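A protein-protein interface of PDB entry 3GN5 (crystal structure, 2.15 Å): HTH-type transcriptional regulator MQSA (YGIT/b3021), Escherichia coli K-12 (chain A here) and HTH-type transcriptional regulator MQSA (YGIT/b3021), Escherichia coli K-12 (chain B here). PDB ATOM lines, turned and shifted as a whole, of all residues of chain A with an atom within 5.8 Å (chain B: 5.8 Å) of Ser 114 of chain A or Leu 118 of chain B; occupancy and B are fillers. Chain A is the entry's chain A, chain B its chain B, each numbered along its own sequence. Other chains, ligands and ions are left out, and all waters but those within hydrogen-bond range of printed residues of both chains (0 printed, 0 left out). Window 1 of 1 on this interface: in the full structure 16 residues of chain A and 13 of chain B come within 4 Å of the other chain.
ND1 of His 112 of chain A lies close to N of Ser 114 of chain A.
A ring nitrogen (ND1) of His 112 of chain B is in hydrogen-bond range of the backbone NH (N) of Ser 114 of chain B (2.9 Å).
Hydrophobic or aromatic side chains of chain B that line the printed part of chain A: Phe 94, His 112, Leu 118, Val 121 and Ile 132.
Of the 10 printed residues of chain A, 8 touch a printed residue of chain B.
Among the printed residues, 19 pairs touch across the chains.
Of the printed residues of chain B, Pro 113 of chain A touches Phe 94.
Ser 114 of chain A touches four residues of chain B.
Of the printed residues of chain B, Thr 115 of chain A touches His 112 (3.9 Å) and Ser 114 (2.7 Å).
Printed residues of chain B within 4 Å of Lys 117 of chain A: Ile 93, Leu 118 and Ile 132.
Printed residues of chain B within 4 Å of Ile 132 of chain A: Lys 117 (3.6 Å) and Val 121 (3.4 Å).
Of chain A, only Ser 114, Lys 117 and Leu 118 come within 4 Å of Leu 118 of chain B.
Printed residues of chain A within 4 Å of Val 121 of chain B: Ile 132 (3.4 Å).
The nearest residue of chain B that does not touch Ser 114 of chain A is Gly 95 of chain B (4.6 Å).
Among the printed residues, merely in contact across the chains: His 112 of chain A with Phe 94 of chain B, His 112 of chain A with His 112 of chain B, His 112 of chain A with Thr 115 of chain B, Pro 113 of chain A with Phe 94 of chain B, Ser 114 of chain A with Ser 114 of chain B, Ser 114 of chain A with Leu 118 of chain B, Thr 115 of chain A with His 112 of chain B, Lys 117 of chain A with Leu 118 of chain B, Lys 117 of chain A with Ile 132 of chain B, Leu 118 of chain A with Ser 114 of chain B, Leu 118 of chain A with Lys 117 of chain B, Leu 118 of chain A with Leu 118 of chain B, Val 121 of chain A with Ile 132 of chain B, Ile 132 of chain A with Lys 117 of chain B and Ile 132 of chain A with Val 121 of chain B.
OG of Ser 114 of chain A is in hydrogen-bond range of O of Phe 94 of chain B, 2.5 Å away.
OG of Ser 114 of chain A is in hydrogen-bond range of OG1 of Thr 115 of chain B, 2.5 Å away.
The side-chain hydroxyl (OG) of Ser 114 of chain B is in hydrogen-bond range of the side-chain hydroxyl (OG1) of Thr 115 of chain A (2.7 Å).
The side-chain amino group of Lys 117 of chain A lies within hydrogen-bond range of the backbone carbonyl oxygen of Ile 93 of chain B (3.0 Å).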
ATOM      1  N   HIS A 112       2.778  -2.377   8.762  1.00  0.00           N
ATOM      2  CA  HIS A 112       2.518  -2.744   7.389  1.00  0.00           C
ATOM      3  C   HIS A 112       3.754  -2.317   6.554  1.00  0.00           C
ATOM      4  O   HIS A 112       4.383  -1.301   6.848  1.00  0.00           O
ATOM      5  CB  HIS A 112       1.256  -2.018   6.940  1.00  0.00           C
ATOM      6  CG  HIS A 112       0.752  -2.407   5.592  1.00  0.00           C
ATOM      7  ND1 HIS A 112       1.216  -1.831   4.432  1.00  0.00           N
ATOM      8  CD2 HIS A 112      -0.254  -3.233   5.227  1.00  0.00           C
ATOM      9  CE1 HIS A 112       0.564  -2.336   3.402  1.00  0.00           C
ATOM     10  NE2 HIS A 112      -0.343  -3.183   3.858  1.00  0.00           N
ATOM     11  N   PRO A 113       4.129  -3.116   5.540  1.00  0.00           N
ATOM     12  CA  PRO A 113       5.239  -2.746   4.681  1.00  0.00           C
ATOM     13  C   PRO A 113       5.231  -1.286   4.196  1.00  0.00           C
ATOM     14  O   PRO A 113       6.297  -0.716   4.027  1.00  0.00           O
ATOM     15  CB  PRO A 113       5.082  -3.704   3.490  1.00  0.00           C
ATOM     16  CG  PRO A 113       4.536  -4.926   4.118  1.00  0.00           C
ATOM     17  CD  PRO A 113       3.585  -4.442   5.179  1.00  0.00           C
ATOM     18  N   SER A 114       4.046  -0.712   3.941  1.00  0.00           N
ATOM     19  CA  SER A 114       3.928   0.682   3.467  1.00  0.00           C
ATOM     20  C   SER A 114       4.203   1.716   4.566  1.00  0.00           C
ATOM     21  O   SER A 114       4.699   2.819   4.274  1.00  0.00           O
ATOM     22  CB  SER A 114       2.557   0.944   2.819  1.00  0.00           C
ATOM     23  OG  SER A 114       2.458   0.364   1.527  1.00  0.00           O
ATOM     24  N   THR A 115       3.880   1.374   5.819  1.00  0.00           N
ATOM     25  CA  THR A 115       4.249   2.212   6.968  1.00  0.00           C
ATOM     26  C   THR A 115       5.789   2.257   7.137  1.00  0.00           C
ATOM     27  O   THR A 115       6.369   3.321   7.363  1.00  0.00           O
ATOM     28  CB  THR A 115       3.607   1.691   8.295  1.00  0.00           C
ATOM     29  OG1 THR A 115       2.202   1.499   8.124  1.00  0.00           O
ATOM     30  CG2 THR A 115       3.854   2.630   9.482  1.00  0.00           C
ATOM     31  N   ILE A 116       6.438   1.085   7.043  1.00  0.00           N
ATOM     32  CA  ILE A 116       7.888   0.987   7.132  1.00  0.00           C
ATOM     33  C   ILE A 116       8.532   1.842   6.037  1.00  0.00           C
ATOM     34  O   ILE A 116       9.460   2.607   6.282  1.00  0.00           O
ATOM     35  CB  ILE A 116       8.389  -0.489   6.968  1.00  0.00           C
ATOM     36  CG1 ILE A 116       7.854  -1.394   8.082  1.00  0.00           C
ATOM     37  CG2 ILE A 116       9.945  -0.518   6.922  1.00  0.00           C
ATOM     38  CD1 ILE A 116       8.260  -2.878   7.981  1.00  0.00           C
ATOM     39  N   LYS A 117       8.043   1.685   4.812  1.00  0.00           N
ATOM     40  CA  LYS A 117       8.578   2.429   3.683  1.00  0.00           C
ATOM     41  C   LYS A 117       8.342   3.929   3.782  1.00  0.00           C
ATOM     42  O   LYS A 117       9.239   4.715   3.484  1.00  0.00           O
ATOM     43  CB  LYS A 117       8.068   1.832   2.375  1.00  0.00           C
ATOM     44  CG  LYS A 117       8.761   0.517   2.101  1.00  0.00           C
ATOM     45  CD  LYS A 117       8.244  -0.199   0.881  1.00  0.00           C
ATOM     46  CE  LYS A 117       9.213  -1.337   0.453  1.00  0.00           C
ATOM     47  NZ  LYS A 117       8.890  -2.648   1.086  1.00  0.00           N
ATOM     48  N   LEU A 118       7.156   4.322   4.223  1.00  0.00           N
ATOM     49  CA  LEU A 118       6.864   5.741   4.529  1.00  0.00           C
ATOM     50  C   LEU A 118       7.829   6.286   5.618  1.00  0.00           C
ATOM     51  O   LEU A 118       8.395   7.360   5.470  1.00  0.00           O
ATOM     52  CB  LEU A 118       5.394   5.864   4.948  1.00  0.00           C
ATOM     53  CG  LEU A 118       4.611   7.166   4.804  1.00  0.00           C
ATOM     54  CD1 LEU A 118       4.871   7.842   3.492  1.00  0.00           C
ATOM     55  CD2 LEU A 118       3.113   6.860   5.021  1.00  0.00           C
ATOM     56  N   LEU A 119       8.084   5.501   6.660  1.00  0.00           N
ATOM     57  CA  LEU A 119       9.076   5.880   7.674  1.00  0.00           C
ATOM     58  C   LEU A 119      10.468   6.068   7.097  1.00  0.00           C
ATOM     59  O   LEU A 119      11.161   7.022   7.446  1.00  0.00           O
ATOM     60  CB  LEU A 119       9.123   4.855   8.813  1.00  0.00           C
ATOM     61  CG  LEU A 119       7.968   4.939   9.819  1.00  0.00           C
ATOM     62  CD1 LEU A 119       7.852   3.643  10.629  1.00  0.00           C
ATOM     63  CD2 LEU A 119       8.112   6.174  10.742  1.00  0.00           C
ATOM     64  N   VAL A 121      11.268   6.890   3.984  1.00  0.00           N
ATOM     65  CA  VAL A 121      11.251   8.110   3.180  1.00  0.00           C
ATOM     66  C   VAL A 121      11.214   9.387   4.016  1.00  0.00           C
ATOM     67  O   VAL A 121      11.897  10.358   3.684  1.00  0.00           O
ATOM     68  CB  VAL A 121      10.021   8.119   2.262  1.00  0.00           C
ATOM     69  CG1 VAL A 121       9.881   9.486   1.549  1.00  0.00           C
ATOM     70  CG2 VAL A 121      10.084   6.945   1.276  1.00  0.00           C
ATOM     71  N   ILE A 132       1.612  14.130   4.110  1.00  0.00           N
ATOM     72  CA  ILE A 132       0.941  12.943   4.662  1.00  0.00           C
ATOM     73  C   ILE A 132       0.125  13.192   5.929  1.00  0.00           C
ATOM     74  O   ILE A 132      -0.553  12.279   6.384  1.00  0.00           O
ATOM     75  CB  ILE A 132       1.943  11.762   4.890  1.00  0.00           C
ATOM     76  CG1 ILE A 132       2.941  12.070   6.014  1.00  0.00           C
ATOM     77  CG2 ILE A 132       2.686  11.464   3.596  1.00  0.00           C
ATOM     78  CD1 ILE A 132       3.781  10.863   6.426  1.00  0.00           C
ATOM     79  N   ILE B  93       6.271  -4.327  -3.471  1.00  0.00           N
ATOM     80  CA  ILE B  93       6.892  -3.117  -2.960  1.00  0.00           C
ATOM     81  C   ILE B  93       6.040  -2.537  -1.829  1.00  0.00           C
ATOM     82  O   ILE B  93       6.539  -2.255  -0.729  1.00  0.00           O
ATOM     83  CB  ILE B  93       7.109  -2.065  -4.110  1.00  0.00           C
ATOM     84  CG1 ILE B  93       8.148  -2.556  -5.129  1.00  0.00           C
ATOM     85  CG2 ILE B  93       7.583  -0.759  -3.561  1.00  0.00           C
ATOM     86  CD1 ILE B  93       8.120  -1.806  -6.471  1.00  0.00           C
ATOM     87  N   PHE B  94       4.750  -2.367  -2.099  1.00  0.00           N
ATOM     88  CA  PHE B  94       3.867  -1.619  -1.193  1.00  0.00           C
ATOM     89  C   PHE B  94       3.203  -2.509  -0.135  1.00  0.00           C
ATOM     90  O   PHE B  94       2.889  -2.036   0.970  1.00  0.00           O
ATOM     91  CB  PHE B  94       2.821  -0.839  -1.996  1.00  0.00           C
ATOM     92  CG  PHE B  94       3.418   0.212  -2.891  1.00  0.00           C
ATOM     93  CD1 PHE B  94       3.902   1.394  -2.361  1.00  0.00           C
ATOM     94  CD2 PHE B  94       3.511   0.013  -4.265  1.00  0.00           C
ATOM     95  CE1 PHE B  94       4.465   2.360  -3.184  1.00  0.00           C
ATOM     96  CE2 PHE B  94       4.072   0.977  -5.092  1.00  0.00           C
ATOM     97  CZ  PHE B  94       4.551   2.146  -4.552  1.00  0.00           C
ATOM     98  N   GLY B  95       3.011  -3.788  -0.467  1.00  0.00           N
ATOM     99  CA  GLY B  95       2.426  -4.757   0.458  1.00  0.00           C
ATOM    100  C   GLY B  95       0.953  -4.969   0.163  1.00  0.00           C
ATOM    101  O   GLY B  95       0.436  -4.449  -0.820  1.00  0.00           O
ATOM    102  N   HIS B 112      -4.063  -0.253   2.129  1.00  0.00           N
ATOM    103  CA  HIS B 112      -3.805   0.212   3.491  1.00  0.00           C
ATOM    104  C   HIS B 112      -3.659   1.749   3.469  1.00  0.00           C
ATOM    105  O   HIS B 112      -3.192   2.319   2.468  1.00  0.00           O
ATOM    106  CB  HIS B 112      -2.548  -0.461   4.039  1.00  0.00           C
ATOM    107  CG  HIS B 112      -2.281  -0.190   5.490  1.00  0.00           C
ATOM    108  ND1 HIS B 112      -1.637   0.947   5.928  1.00  0.00           N
ATOM    109  CD2 HIS B 112      -2.556  -0.918   6.600  1.00  0.00           C
ATOM    110  CE1 HIS B 112      -1.558   0.927   7.245  1.00  0.00           C
ATOM    111  NE2 HIS B 112      -2.089  -0.204   7.676  1.00  0.00           N
ATOM    112  N   PRO B 113      -4.083   2.433   4.556  1.00  0.00           N
ATOM    113  CA  PRO B 113      -3.908   3.889   4.601  1.00  0.00           C
ATOM    114  C   PRO B 113      -2.486   4.364   4.322  1.00  0.00           C
ATOM    115  O   PRO B 113      -2.323   5.377   3.658  1.00  0.00           O
ATOM    116  CB  PRO B 113      -4.343   4.251   6.031  1.00  0.00           C
ATOM    117  CG  PRO B 113      -5.341   3.215   6.379  1.00  0.00           C
ATOM    118  CD  PRO B 113      -4.798   1.938   5.750  1.00  0.00           C
ATOM    119  N   SER B 114      -1.470   3.631   4.798  1.00  0.00           N
ATOM    120  CA  SER B 114      -0.059   3.972   4.534  1.00  0.00           C
ATOM    121  C   SER B 114       0.326   3.816   3.064  1.00  0.00           C
ATOM    122  O   SER B 114       1.162   4.553   2.558  1.00  0.00           O
ATOM    123  CB  SER B 114       0.891   3.113   5.402  1.00  0.00           C
ATOM    124  OG  SER B 114       0.705   3.355   6.788  1.00  0.00           O
ATOM    125  N   THR B 115      -0.237   2.824   2.383  1.00  0.00           N
ATOM    126  CA  THR B 115       0.007   2.661   0.948  1.00  0.00           C
ATOM    127  C   THR B 115      -0.589   3.827   0.135  1.00  0.00           C
ATOM    128  O   THR B 115       0.042   4.337  -0.779  1.00  0.00           O
ATOM    129  CB  THR B 115      -0.593   1.356   0.400  1.00  0.00           C
ATOM    130  OG1 THR B 115      -0.053   0.225   1.108  1.00  0.00           O
ATOM    131  CG2 THR B 115      -0.285   1.251  -1.075  1.00  0.00           C
ATOM    132  N   ILE B 116      -1.809   4.227   0.463  1.00  0.00           N
ATOM    133  CA  ILE B 116      -2.437   5.434  -0.138  1.00  0.00           C
ATOM    134  C   ILE B 116      -1.529   6.640   0.036  1.00  0.00           C
ATOM    135  O   ILE B 116      -1.173   7.297  -0.928  1.00  0.00           O
ATOM    136  CB  ILE B 116      -3.805   5.729   0.502  1.00  0.00           C
ATOM    137  CG1 ILE B 116      -4.793   4.600   0.201  1.00  0.00           C
ATOM    138  CG2 ILE B 116      -4.368   7.063   0.020  1.00  0.00           C
ATOM    139  CD1 ILE B 116      -6.026   4.651   1.069  1.00  0.00           C
ATOM    140  N   LYS B 117      -1.130   6.903   1.275  1.00  0.00           N
ATOM    141  CA  LYS B 117      -0.210   8.001   1.575  1.00  0.00           C
ATOM    142  C   LYS B 117       1.089   7.898   0.790  1.00  0.00           C
ATOM    143  O   LYS B 117       1.569   8.899   0.261  1.00  0.00           O
ATOM    144  CB  LYS B 117       0.099   8.047   3.070  1.00  0.00           C
ATOM    145  CG  LYS B 117      -0.966   8.748   3.900  1.00  0.00           C
ATOM    146  CD  LYS B 117      -1.058   8.199   5.313  1.00  0.00           C
ATOM    147  CE  LYS B 117      -2.045   9.036   6.148  1.00  0.00           C
ATOM    148  NZ  LYS B 117      -2.324   8.434   7.480  1.00  0.00           N
ATOM    149  N   LEU B 118       1.659   6.689   0.726  1.00  0.00           N
ATOM    150  CA  LEU B 118       2.903   6.455  -0.004  1.00  0.00           C
ATOM    151  C   LEU B 118       2.715   6.697  -1.526  1.00  0.00           C
ATOM    152  O   LEU B 118       3.569   7.313  -2.186  1.00  0.00           O
ATOM    153  CB  LEU B 118       3.434   5.035   0.309  1.00  0.00           C
ATOM    154  CG  LEU B 118       4.856   4.650  -0.083  1.00  0.00           C
ATOM    155  CD1 LEU B 118       5.831   5.683   0.426  1.00  0.00           C
ATOM    156  CD2 LEU B 118       5.229   3.250   0.446  1.00  0.00           C
ATOM    157  N   LEU B 119       1.574   6.262  -2.067  1.00  0.00           N
ATOM    158  CA  LEU B 119       1.212   6.527  -3.477  1.00  0.00           C
ATOM    159  C   LEU B 119       0.896   7.997  -3.782  1.00  0.00           C
ATOM    160  O   LEU B 119       1.205   8.480  -4.873  1.00  0.00           O
ATOM    161  CB  LEU B 119       0.014   5.678  -3.884  1.00  0.00           C
ATOM    162  CG  LEU B 119       0.252   4.172  -4.026  1.00  0.00           C
ATOM    163  CD1 LEU B 119      -1.079   3.457  -4.229  1.00  0.00           C
ATOM    164  CD2 LEU B 119       1.209   3.895  -5.180  1.00  0.00           C
ATOM    165  N   ARG B 120       0.262   8.703  -2.846  1.00  0.00           N
ATOM    166  CA  ARG B 120       0.042  10.154  -3.012  1.00  0.00           C
ATOM    167  C   ARG B 120       1.367  10.903  -2.988  1.00  0.00           C
ATOM    168  O   ARG B 120       1.592  11.792  -3.798  1.00  0.00           O
ATOM    169  CB  ARG B 120      -0.925  10.726  -1.959  1.00  0.00           C
ATOM    170  CG  ARG B 120      -2.373  10.586  -2.365  1.00  0.00           C
ATOM    171  CD  ARG B 120      -3.374  11.244  -1.390  1.00  0.00           C
ATOM    172  NE  ARG B 120      -4.621  10.472  -1.370  1.00  0.00           N
ATOM    173  CZ  ARG B 120      -5.481  10.389  -2.388  1.00  0.00           C
ATOM    174  NH1 ARG B 120      -5.265  11.050  -3.523  1.00  0.00           N
ATOM    175  NH2 ARG B 120      -6.569   9.635  -2.280  1.00  0.00           N
ATOM    176  N   VAL B 121       2.245  10.531  -2.066  1.00  0.00           N
ATOM    177  CA  VAL B 121       3.598  11.092  -2.024  1.00  0.00           C
ATOM    178  C   VAL B 121       4.337  10.832  -3.336  1.00  0.00           C
ATOM    179  O   VAL B 121       4.957  11.735  -3.904  1.00  0.00           O
ATOM    180  CB  VAL B 121       4.408  10.534  -0.830  1.00  0.00           C
ATOM    181  CG1 VAL B 121       5.910  10.838  -0.983  1.00  0.00           C
ATOM    182  CG2 VAL B 121       3.868  11.104   0.480  1.00  0.00           C
ATOM    183  N   LEU B 122       4.252   9.600  -3.825  1.00  0.00           N
ATOM    184  CA  LEU B 122       4.993   9.198  -5.021  1.00  0.00           C
ATOM    185  C   LEU B 122       4.450   9.840  -6.292  1.00  0.00           C
ATOM    186  O   LEU B 122       5.202  10.063  -7.237  1.00  0.00           O
ATOM    187  CB  LEU B 122       5.028   7.672  -5.153  1.00  0.00           C
ATOM    188  CG  LEU B 122       5.958   7.019  -4.131  1.00  0.00           C
ATOM    189  CD1 LEU B 122       5.660   5.510  -4.001  1.00  0.00           C
ATOM    190  CD2 LEU B 122       7.400   7.287  -4.495  1.00  0.00           C
ATOM    191  N   ASP B 123       3.151  10.121  -6.311  1.00  0.00           N
ATOM    192  CA  ASP B 123       2.523  10.870  -7.397  1.00  0.00           C
ATOM    193  C   ASP B 123       3.174  12.233  -7.577  1.00  0.00           C
ATOM    194  O   ASP B 123       3.368  12.677  -8.715  1.00  0.00           O
ATOM    195  CB  ASP B 123       1.016  11.057  -7.128  1.00  0.00           C
ATOM    196  CG  ASP B 123       0.276  11.681  -8.306  1.00  0.00           C
ATOM    197  OD1 ASP B 123       0.451  11.223  -9.462  1.00  0.00           O
ATOM    198  OD2 ASP B 123      -0.498  12.625  -8.073  1.00  0.00           O
ATOM    199  N   ILE B 132      12.826   3.253  -1.835  1.00  0.00           N
ATOM    200  CA  ILE B 132      12.114   2.159  -1.150  1.00  0.00           C
ATOM    201  C   ILE B 132      11.804   0.917  -2.027  1.00  0.00           C
ATOM    202  O   ILE B 132      11.180  -0.032  -1.565  1.00  0.00           O
ATOM    203  CB  ILE B 132      10.865   2.687  -0.392  1.00  0.00           C
ATOM    204  CG1 ILE B 132       9.855   3.387  -1.322  1.00  0.00           C
ATOM    205  CG2 ILE B 132      11.323   3.645   0.704  1.00  0.00           C
ATOM    206  CD1 ILE B 132       8.754   2.488  -1.850  1.00  0.00           C
